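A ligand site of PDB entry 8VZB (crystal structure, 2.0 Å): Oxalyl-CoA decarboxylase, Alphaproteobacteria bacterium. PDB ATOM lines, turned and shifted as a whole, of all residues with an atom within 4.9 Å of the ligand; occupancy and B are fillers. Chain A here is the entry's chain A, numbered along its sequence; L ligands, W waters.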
ATOM      1  N   ASN A 101       2.961  -5.644  20.918  1.00  0.00           N
ATOM      2  CA  ASN A 101       3.178  -6.908  20.226  1.00  0.00           C
ATOM      3  C   ASN A 101       3.538  -6.728  18.759  1.00  0.00           C
ATOM      4  O   ASN A 101       3.780  -7.737  18.071  1.00  0.00           O
ATOM      5  CB  ASN A 101       1.936  -7.802  20.342  1.00  0.00           C
ATOM      6  CG  ASN A 101       1.803  -8.425  21.715  1.00  0.00           C
ATOM      7  OD1 ASN A 101       2.478  -9.407  22.033  1.00  0.00           O
ATOM      8  ND2 ASN A 101       0.919  -7.875  22.532  1.00  0.00           N
ATOM      9  N   CYS A 102       3.577  -5.496  18.251  1.00  0.00           N
ATOM     10  CA  CYS A 102       3.829  -5.227  16.832  1.00  0.00           C
ATOM     11  C   CYS A 102       2.790  -5.930  15.951  1.00  0.00           C
ATOM     12  O   CYS A 102       3.115  -6.477  14.900  1.00  0.00           O
ATOM     13  CB  CYS A 102       5.248  -5.626  16.414  1.00  0.00           C
ATOM     14  SG  CYS A 102       6.555  -4.885  17.431  1.00  0.00           S
ATOM     15  N   ARG A 162       7.279  -2.063  10.669  1.00  0.00           N
ATOM     16  CA  ARG A 162       6.938  -2.708  11.928  1.00  0.00           C
ATOM     17  C   ARG A 162       5.457  -2.488  12.194  1.00  0.00           C
ATOM     18  O   ARG A 162       5.043  -1.332  12.364  1.00  0.00           O
ATOM     19  CB  ARG A 162       7.778  -2.165  13.069  1.00  0.00           C
ATOM     20  CG  ARG A 162       7.380  -2.718  14.429  1.00  0.00           C
ATOM     21  CD  ARG A 162       8.229  -2.136  15.535  1.00  0.00           C
ATOM     22  NE  ARG A 162       9.251  -3.064  15.994  1.00  0.00           N
ATOM     23  CZ  ARG A 162      10.045  -2.850  17.025  1.00  0.00           C
ATOM     24  NH1 ARG A 162       9.990  -1.715  17.717  1.00  0.00           N
ATOM     25  NH2 ARG A 162      10.929  -3.780  17.369  1.00  0.00           N
ATOM     26  N   PRO A 163       4.628  -3.523  12.217  1.00  0.00           N
ATOM     27  CA  PRO A 163       3.179  -3.308  12.310  1.00  0.00           C
ATOM     28  C   PRO A 163       2.780  -2.657  13.624  1.00  0.00           C
ATOM     29  O   PRO A 163       3.481  -2.743  14.639  1.00  0.00           O
ATOM     30  CB  PRO A 163       2.596  -4.730  12.188  1.00  0.00           C
ATOM     31  CG  PRO A 163       3.681  -5.527  11.516  1.00  0.00           C
ATOM     32  CD  PRO A 163       4.961  -4.950  12.045  1.00  0.00           C
ATOM     33  N   GLY A 221      11.041 -16.461  17.092  1.00  0.00           N
ATOM     34  CA  GLY A 221      10.040 -15.613  17.694  1.00  0.00           C
ATOM     35  C   GLY A 221       8.817 -15.429  16.797  1.00  0.00           C
ATOM     36  O   GLY A 221       8.770 -15.856  15.653  1.00  0.00           O
ATOM     37  N   LYS A 222       7.805 -14.742  17.362  1.00  0.00           N
ATOM     38  CA  LYS A 222       6.558 -14.583  16.633  1.00  0.00           C
ATOM     39  C   LYS A 222       6.682 -13.587  15.481  1.00  0.00           C
ATOM     40  O   LYS A 222       5.763 -13.515  14.644  1.00  0.00           O
ATOM     41  CB  LYS A 222       5.431 -14.160  17.580  1.00  0.00           C
ATOM     42  CG  LYS A 222       5.507 -12.740  18.135  1.00  0.00           C
ATOM     43  CD  LYS A 222       4.206 -12.401  18.872  1.00  0.00           C
ATOM     44  CE  LYS A 222       4.150 -10.940  19.311  1.00  0.00           C
ATOM     45  NZ  LYS A 222       4.867 -10.694  20.592  1.00  0.00           N
ATOM     46  N   GLY A 223       7.784 -12.831  15.397  1.00  0.00           N
ATOM     47  CA  GLY A 223       8.034 -12.057  14.200  1.00  0.00           C
ATOM     48  C   GLY A 223       8.151 -12.933  12.960  1.00  0.00           C
ATOM     49  O   GLY A 223       7.758 -12.516  11.861  1.00  0.00           O
ATOM     50  N   TRP A 226       4.495 -13.806  12.134  1.00  0.00           N
ATOM     51  CA  TRP A 226       3.856 -12.705  11.421  1.00  0.00           C
ATOM     52  C   TRP A 226       4.345 -12.626   9.980  1.00  0.00           C
ATOM     53  O   TRP A 226       3.565 -12.390   9.053  1.00  0.00           O
ATOM     54  CB  TRP A 226       4.112 -11.384  12.126  1.00  0.00           C
ATOM     55  CG  TRP A 226       3.783 -10.256  11.225  1.00  0.00           C
ATOM     56  CD1 TRP A 226       4.662  -9.465  10.543  1.00  0.00           C
ATOM     57  CD2 TRP A 226       2.477  -9.838  10.831  1.00  0.00           C
ATOM     58  NE1 TRP A 226       3.974  -8.563   9.771  1.00  0.00           N
ATOM     59  CE2 TRP A 226       2.635  -8.766   9.929  1.00  0.00           C
ATOM     60  CE3 TRP A 226       1.178 -10.253  11.167  1.00  0.00           C
ATOM     61  CZ2 TRP A 226       1.557  -8.104   9.364  1.00  0.00           C
ATOM     62  CZ3 TRP A 226       0.109  -9.596  10.592  1.00  0.00           C
ATOM     63  CH2 TRP A 226       0.301  -8.542   9.709  1.00  0.00           C
ATOM     64  N   SER A 227       5.650 -12.832   9.769  1.00  0.00           N
ATOM     65  CA  SER A 227       6.246 -12.724   8.453  1.00  0.00           C
ATOM     66  C   SER A 227       5.856 -13.868   7.529  1.00  0.00           C
ATOM     67  O   SER A 227       6.193 -13.815   6.330  1.00  0.00           O
ATOM     68  CB  SER A 227       7.774 -12.671   8.585  1.00  0.00           C
ATOM     69  OG  SER A 227       8.402 -12.582   7.318  1.00  0.00           O
ATOM     70  N   THR A 247       9.895 -19.016  21.208  1.00  0.00           N
ATOM     71  CA  THR A 247       9.288 -18.092  22.154  1.00  0.00           C
ATOM     72  C   THR A 247       7.843 -18.520  22.393  1.00  0.00           C
ATOM     73  O   THR A 247       7.320 -19.387  21.682  1.00  0.00           O
ATOM     74  CB  THR A 247       9.365 -16.665  21.615  1.00  0.00           C
ATOM     75  OG1 THR A 247       8.528 -16.547  20.455  1.00  0.00           O
ATOM     76  CG2 THR A 247      10.804 -16.305  21.258  1.00  0.00           C
ATOM     77  N   GLY A 250       6.008 -17.851  19.345  1.00  0.00           N
ATOM     78  CA  GLY A 250       6.739 -18.463  18.251  1.00  0.00           C
ATOM     79  C   GLY A 250       6.562 -19.967  18.148  1.00  0.00           C
ATOM     80  O   GLY A 250       7.017 -20.569  17.169  1.00  0.00           O
ATOM     81  N   GLY A 280      13.314 -12.763  14.549  1.00  0.00           N
ATOM     82  CA  GLY A 280      12.058 -12.078  14.857  1.00  0.00           C
ATOM     83  C   GLY A 280      11.648 -12.208  16.304  1.00  0.00           C
ATOM     84  O   GLY A 280      10.481 -12.464  16.608  1.00  0.00           O
ATOM     85  N   ALA A 281      12.614 -12.079  17.215  1.00  0.00           N
ATOM     86  CA  ALA A 281      12.372 -12.100  18.650  1.00  0.00           C
ATOM     87  C   ALA A 281      13.220 -11.020  19.300  1.00  0.00           C
ATOM     88  O   ALA A 281      14.351 -10.775  18.869  1.00  0.00           O
ATOM     89  CB  ALA A 281      12.705 -13.467  19.259  1.00  0.00           C
ATOM     90  N   ARG A 282      12.681 -10.368  20.320  1.00  0.00           N
ATOM     91  CA  ARG A 282      13.371  -9.273  20.979  1.00  0.00           C
ATOM     92  C   ARG A 282      14.060  -9.734  22.255  1.00  0.00           C
ATOM     93  O   ARG A 282      13.614 -10.659  22.927  1.00  0.00           O
ATOM     94  CB  ARG A 282      12.407  -8.130  21.307  1.00  0.00           C
ATOM     95  CG  ARG A 282      12.062  -7.261  20.126  1.00  0.00           C
ATOM     96  CD  ARG A 282      10.999  -6.260  20.505  1.00  0.00           C
ATOM     97  NE  ARG A 282       9.727  -6.913  20.810  1.00  0.00           N
ATOM     98  CZ  ARG A 282       8.581  -6.273  20.973  1.00  0.00           C
ATOM     99  NH1 ARG A 282       8.506  -4.957  20.910  1.00  0.00           N
ATOM    100  NH2 ARG A 282       7.475  -6.976  21.206  1.00  0.00           N
ATOM    101  N   ASN A 284      13.801  -8.506  25.050  1.00  0.00           N
ATOM    102  CA  ASN A 284      13.025  -7.866  26.099  1.00  0.00           C
ATOM    103  C   ASN A 284      12.859  -8.855  27.250  1.00  0.00           C
ATOM    104  O   ASN A 284      13.608  -9.847  27.342  1.00  0.00           O
ATOM    105  CB  ASN A 284      11.691  -7.356  25.526  1.00  0.00           C
ATOM    106  CG  ASN A 284      10.750  -8.480  25.098  1.00  0.00           C
ATOM    107  OD1 ASN A 284      11.096  -9.667  25.174  1.00  0.00           O
ATOM    108  ND2 ASN A 284       9.564  -8.118  24.657  1.00  0.00           N
ATOM    109  N   ILE A 286      10.766 -11.174  27.823  1.00  0.00           N
ATOM    110  CA  ILE A 286      10.416 -12.554  27.490  1.00  0.00           C
ATOM    111  C   ILE A 286      11.674 -13.390  27.222  1.00  0.00           C
ATOM    112  O   ILE A 286      11.699 -14.594  27.513  1.00  0.00           O
ATOM    113  CB  ILE A 286       9.432 -12.578  26.298  1.00  0.00           C
ATOM    114  CG1 ILE A 286       7.992 -12.433  26.806  1.00  0.00           C
ATOM    115  CG2 ILE A 286       9.557 -13.849  25.461  1.00  0.00           C
ATOM    116  CD1 ILE A 286       6.932 -12.473  25.732  1.00  0.00           C
ATOM    117  N   LEU A 287      12.739 -12.768  26.727  1.00  0.00           N
ATOM    118  CA  LEU A 287      14.023 -13.445  26.551  1.00  0.00           C
ATOM    119  C   LEU A 287      15.073 -12.961  27.550  1.00  0.00           C
ATOM    120  O   LEU A 287      16.278 -13.132  27.315  1.00  0.00           O
ATOM    121  CB  LEU A 287      14.524 -13.290  25.116  1.00  0.00           C
ATOM    122  CG  LEU A 287      13.776 -14.160  24.103  1.00  0.00           C
ATOM    123  CD1 LEU A 287      14.241 -13.885  22.689  1.00  0.00           C
ATOM    124  CD2 LEU A 287      13.934 -15.648  24.460  1.00  0.00           C
ATOM    125  N   LEU A 304      18.057 -11.023  13.564  1.00  0.00           N
ATOM    126  CA  LEU A 304      17.190 -10.740  12.424  1.00  0.00           C
ATOM    127  C   LEU A 304      15.954  -9.986  12.922  1.00  0.00           C
ATOM    128  O   LEU A 304      15.156 -10.535  13.693  1.00  0.00           O
ATOM    129  CB  LEU A 304      16.776 -12.032  11.719  1.00  0.00           C
ATOM    130  CG  LEU A 304      16.354 -11.992  10.236  1.00  0.00           C
ATOM    131  CD1 LEU A 304      15.940 -13.385   9.774  1.00  0.00           C
ATOM    132  CD2 LEU A 304      15.233 -10.989   9.952  1.00  0.00           C
ATOM    133  N   ASP A 305      15.801  -8.746  12.480  1.00  0.00           N
ATOM    134  CA  ASP A 305      14.622  -7.976  12.834  1.00  0.00           C
ATOM    135  C   ASP A 305      14.314  -6.982  11.723  1.00  0.00           C
ATOM    136  O   ASP A 305      15.234  -6.452  11.087  1.00  0.00           O
ATOM    137  CB  ASP A 305      14.794  -7.239  14.166  1.00  0.00           C
ATOM    138  CG  ASP A 305      13.454  -6.790  14.755  1.00  0.00           C
ATOM    139  OD1 ASP A 305      12.713  -6.043  14.071  1.00  0.00           O
ATOM    140  OD2 ASP A 305      13.144  -7.190  15.896  1.00  0.00           O
ATOM    141  N   LEU A 306      13.026  -6.749  11.494  1.00  0.00           N
ATOM    142  CA  LEU A 306      12.619  -5.758  10.514  1.00  0.00           C
ATOM    143  C   LEU A 306      12.955  -4.347  10.970  1.00  0.00           C
ATOM    144  O   LEU A 306      13.198  -3.468  10.142  1.00  0.00           O
ATOM    145  CB  LEU A 306      11.110  -5.911  10.242  1.00  0.00           C
ATOM    146  CG  LEU A 306      10.453  -5.036   9.178  1.00  0.00           C
ATOM    147  CD1 LEU A 306      11.226  -5.105   7.873  1.00  0.00           C
ATOM    148  CD2 LEU A 306       9.013  -5.503   8.977  1.00  0.00           C
ATOM    149  N   SER A 307      12.992  -4.122  12.286  1.00  0.00           N
ATOM    150  CA  SER A 307      13.242  -2.805  12.855  1.00  0.00           C
ATOM    151  C   SER A 307      14.731  -2.605  13.092  1.00  0.00           C
ATOM    152  O   SER A 307      15.333  -3.290  13.927  1.00  0.00           O
ATOM    153  CB  SER A 307      12.464  -2.637  14.160  1.00  0.00           C
ATOM    154  OG  SER A 307      12.735  -1.369  14.746  1.00  0.00           O
ATOM    155  N   GLU A 310      15.869  -1.677  16.665  1.00  0.00           N
ATOM    156  CA  GLU A 310      15.878  -2.738  17.672  1.00  0.00           C
ATOM    157  C   GLU A 310      17.221  -3.456  17.764  1.00  0.00           C
ATOM    158  O   GLU A 310      17.496  -4.102  18.785  1.00  0.00           O
ATOM    159  CB  GLU A 310      14.756  -3.748  17.368  1.00  0.00           C
ATOM    160  CG  GLU A 310      14.532  -4.820  18.428  1.00  0.00           C
ATOM    161  CD  GLU A 310      13.913  -4.272  19.706  1.00  0.00           C
ATOM    162  OE1 GLU A 310      13.081  -3.341  19.609  1.00  0.00           O
ATOM    163  OE2 GLU A 310      14.246  -4.779  20.797  1.00  0.00           O
ATOM    164  N   GLY A 323      15.723  -6.556   8.032  1.00  0.00           N
ATOM    165  CA  GLY A 323      14.872  -6.824   6.893  1.00  0.00           C
ATOM    166  C   GLY A 323      13.783  -7.804   7.272  1.00  0.00           C
ATOM    167  O   GLY A 323      13.550  -8.080   8.447  1.00  0.00           O
ATOM    168  N   ASP A 324      13.131  -8.347   6.241  1.00  0.00           N
ATOM    169  CA  ASP A 324      12.006  -9.230   6.451  1.00  0.00           C
ATOM    170  C   ASP A 324      12.477 -10.648   6.789  1.00  0.00           C
ATOM    171  O   ASP A 324      13.448 -11.144   6.209  1.00  0.00           O
ATOM    172  CB  ASP A 324      11.113  -9.259   5.216  1.00  0.00           C
ATOM    173  CG  ASP A 324      10.012 -10.280   5.324  1.00  0.00           C
ATOM    174  OD1 ASP A 324       9.052 -10.051   6.101  1.00  0.00           O
ATOM    175  OD2 ASP A 324      10.104 -11.328   4.644  1.00  0.00           O
ATOM    176  N   GLY A 325      11.772 -11.285   7.722  1.00  0.00           N
ATOM    177  CA  GLY A 325      12.183 -12.608   8.178  1.00  0.00           C
ATOM    178  C   GLY A 325      12.171 -13.649   7.078  1.00  0.00           C
ATOM    179  O   GLY A 325      13.113 -14.448   6.956  1.00  0.00           O
ATOM    180  N   SER A 422       3.427  -9.902  24.773  1.00  0.00           N
ATOM    181  CA  SER A 422       4.524  -9.076  25.255  1.00  0.00           C
ATOM    182  C   SER A 422       4.108  -8.065  26.313  1.00  0.00           C
ATOM    183  O   SER A 422       4.984  -7.495  26.969  1.00  0.00           O
ATOM    184  CB  SER A 422       5.166  -8.352  24.075  1.00  0.00           C
ATOM    185  OG  SER A 422       5.497  -9.248  23.040  1.00  0.00           O
HETATM  186  P1  LIG L   1       8.633 -12.874  20.872  1.00  0.00           P
HETATM  187  O1  LIG L   1       7.625 -12.394  21.888  1.00  0.00           O
HETATM  188  O2  LIG L   1      10.048 -12.940  21.385  1.00  0.00           O
HETATM  189  O3  LIG L   1       8.194 -14.101  20.117  1.00  0.00           O
HETATM  190  P2  LIG L   1       8.689 -10.149  20.032  1.00  0.00           P
HETATM  191  O4  LIG L   1       7.268  -9.640  19.946  1.00  0.00           O
HETATM  192  O5  LIG L   1       9.546  -9.820  21.232  1.00  0.00           O
HETATM  193  O6  LIG L   1       8.685 -11.739  19.740  1.00  0.00           O
HETATM  194  O7  LIG L   1       9.479  -9.626  18.740  1.00  0.00           O
HETATM  195  C1  LIG L   1       8.857  -9.605  17.474  1.00  0.00           C
HETATM  196  C2  LIG L   1       9.819  -8.855  16.561  1.00  0.00           C
HETATM  197  O8  LIG L   1       9.629  -9.252  15.207  1.00  0.00           O
HETATM  198  C3  LIG L   1       9.608  -7.345  16.625  1.00  0.00           C
HETATM  199  O9  LIG L   1      10.808  -6.747  17.094  1.00  0.00           O
HETATM  200  C4  LIG L   1       9.371  -6.915  15.192  1.00  0.00           C
HETATM  201  O10 LIG L   1      10.131  -5.746  14.890  1.00  0.00           O
HETATM  202  C5  LIG L   1       9.874  -8.104  14.395  1.00  0.00           C
HETATM  203  N1  LIG L   1       9.183  -8.228  13.094  1.00  0.00           N
HETATM  204  C6  LIG L   1       7.938  -7.825  12.793  1.00  0.00           C
HETATM  205  N2  LIG L   1       7.644  -8.093  11.498  1.00  0.00           N
HETATM  206  C7  LIG L   1       8.729  -8.681  10.947  1.00  0.00           C
HETATM  207  C8  LIG L   1       9.103  -9.221   9.629  1.00  0.00           C
HETATM  208  N3  LIG L   1       8.214  -9.180   8.600  1.00  0.00           N
HETATM  209  N4  LIG L   1      10.336  -9.752   9.485  1.00  0.00           N
HETATM  210  C9  LIG L   1      11.213  -9.798  10.495  1.00  0.00           C
HETATM  211  N5  LIG L   1      10.943  -9.332  11.733  1.00  0.00           N
HETATM  212  C10 LIG L   1       9.739  -8.769  12.003  1.00  0.00           C
HETATM  213  O   HOH W   1       4.899 -12.670  22.605  1.00  0.00           O
HETATM  214  O   HOH W   2       7.971 -10.180  23.286  1.00  0.00           O
HETATM  215  O   HOH W   3       4.932  -8.213  13.794  1.00  0.00           O
HETATM  216  O   HOH W   4       6.122 -14.712  21.784  1.00  0.00           O
HETATM  217  O   HOH W   5      11.140 -11.736  23.392  1.00  0.00           O
HETATM  218  O   HOH W   6       5.900  -7.609   7.862  1.00  0.00           O
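The side-chain hydroxyl of Thr 247 is in hydrogen-bond range of an oxygen (O3) of the ligand. OD2 of Asp 305 is in hydrogen-bond range of O9 of the ligand (2.7 Å). An oxygen (O3) of the ligand is in hydrogen-bond range of the backbone NH of Lys 222. O4 of the ligand lies within salt-bridge range of NZ of Lys 222 (2.7 Å). The backbone NH (N) of Gly 325 is in hydrogen-bond range of a nitrogen (N4) of the ligand, at 2.7 Å. The side-chain carboxylate of Asp 324 sits at hydrogen-bond distance from a nitrogen (N3) of the ligand (2.8 Å). The backbone NH (N) of Arg 282 is in hydrogen-bond range of an oxygen (O5) of the ligand, 3.3 Å away. NE of Arg 282 is in salt-bridge range of O5 of the ligand (2.9 Å). The guanidinium group of Arg 162 lies within hydrogen-bond range of an oxygen (O9) of the ligand. N5 of the ligand is in hydrogen-bond range of N of Leu 306 (3.3 Å).
Water W5 lies within hydrogen-bond range of an oxygen (O2) of the ligand (2.6 Å), the side-chain amide oxygen of Asn 284 (2.7 Å) and the backbone carbonyl oxygen of Arg 282 (2.7 Å). Water W2 lies within hydrogen-bond range of an oxygen (O5) of the ligand, the side-chain hydroxyl of Ser 422 and the side-chain amide nitrogen of Asn 284. Water W4 bridges O3 of the ligand (2.7 Å) and OG1 of Thr 247 (3.3 Å). Water W1 lies within hydrogen-bond range of NZ of Lys 222 (2.8 Å) and O1 of the ligand (2.8 Å). Water W6 bridges the indole nitrogen of Trp 226 (2.9 Å) and a nitrogen (N3) of the ligand (2.9 Å).
Merely in contact with the ligand: Gly 221, Gly 223, Trp 226, Ser 227, Gly 280, Ala 281, Asn 284, Ile 286, Ser 307, Gly 323 and Ser 422. Hydrophobic or aromatic side chains within 4 Å of the ligand: Trp 226, Ala 281, Ile 286 and Leu 306. Within 4 Å of the ligand: Arg 162, Gly 221, Lys 222, Gly 223, Trp 226, Ser 227, Thr 247, Gly 280, Ala 281, Arg 282, Asn 284, Ile 286, Asp 305, Leu 306, Ser 307, Gly 323, Asp 324, Gly 325 and Ser 422. The nearest printed residue that does not touch the ligand is Cys 102 (4.003 Å).
OG1 of Thr 247 sits at hydrogen-bond distance from N of Gly 250 (3.0 Å). N of Gly 323 sits at hydrogen-bond distance from O of Asp 305 (3.1 Å). OD1 of Asp 305 is in hydrogen-bond range of N of Ser 307, at 2.6 Å. The side-chain hydroxyl (OG) of Ser 422 sits at hydrogen-bond distance from the side-chain amino group (NZ) of Lys 222. The side-chain carboxylate (OD1) of Asp 324 sits at hydrogen-bond distance from the side-chain hydroxyl (OG) of Ser 227 (2.9 Å). NH2 of Arg 162 lies within salt-bridge range of OE1 of Glu 310 (3.1 Å). N of Gly 280 lies within hydrogen-bond range of O of Leu 304. OD1 of Asn 284 sits at hydrogen-bond distance from N of Ile 286 (3.1 Å).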
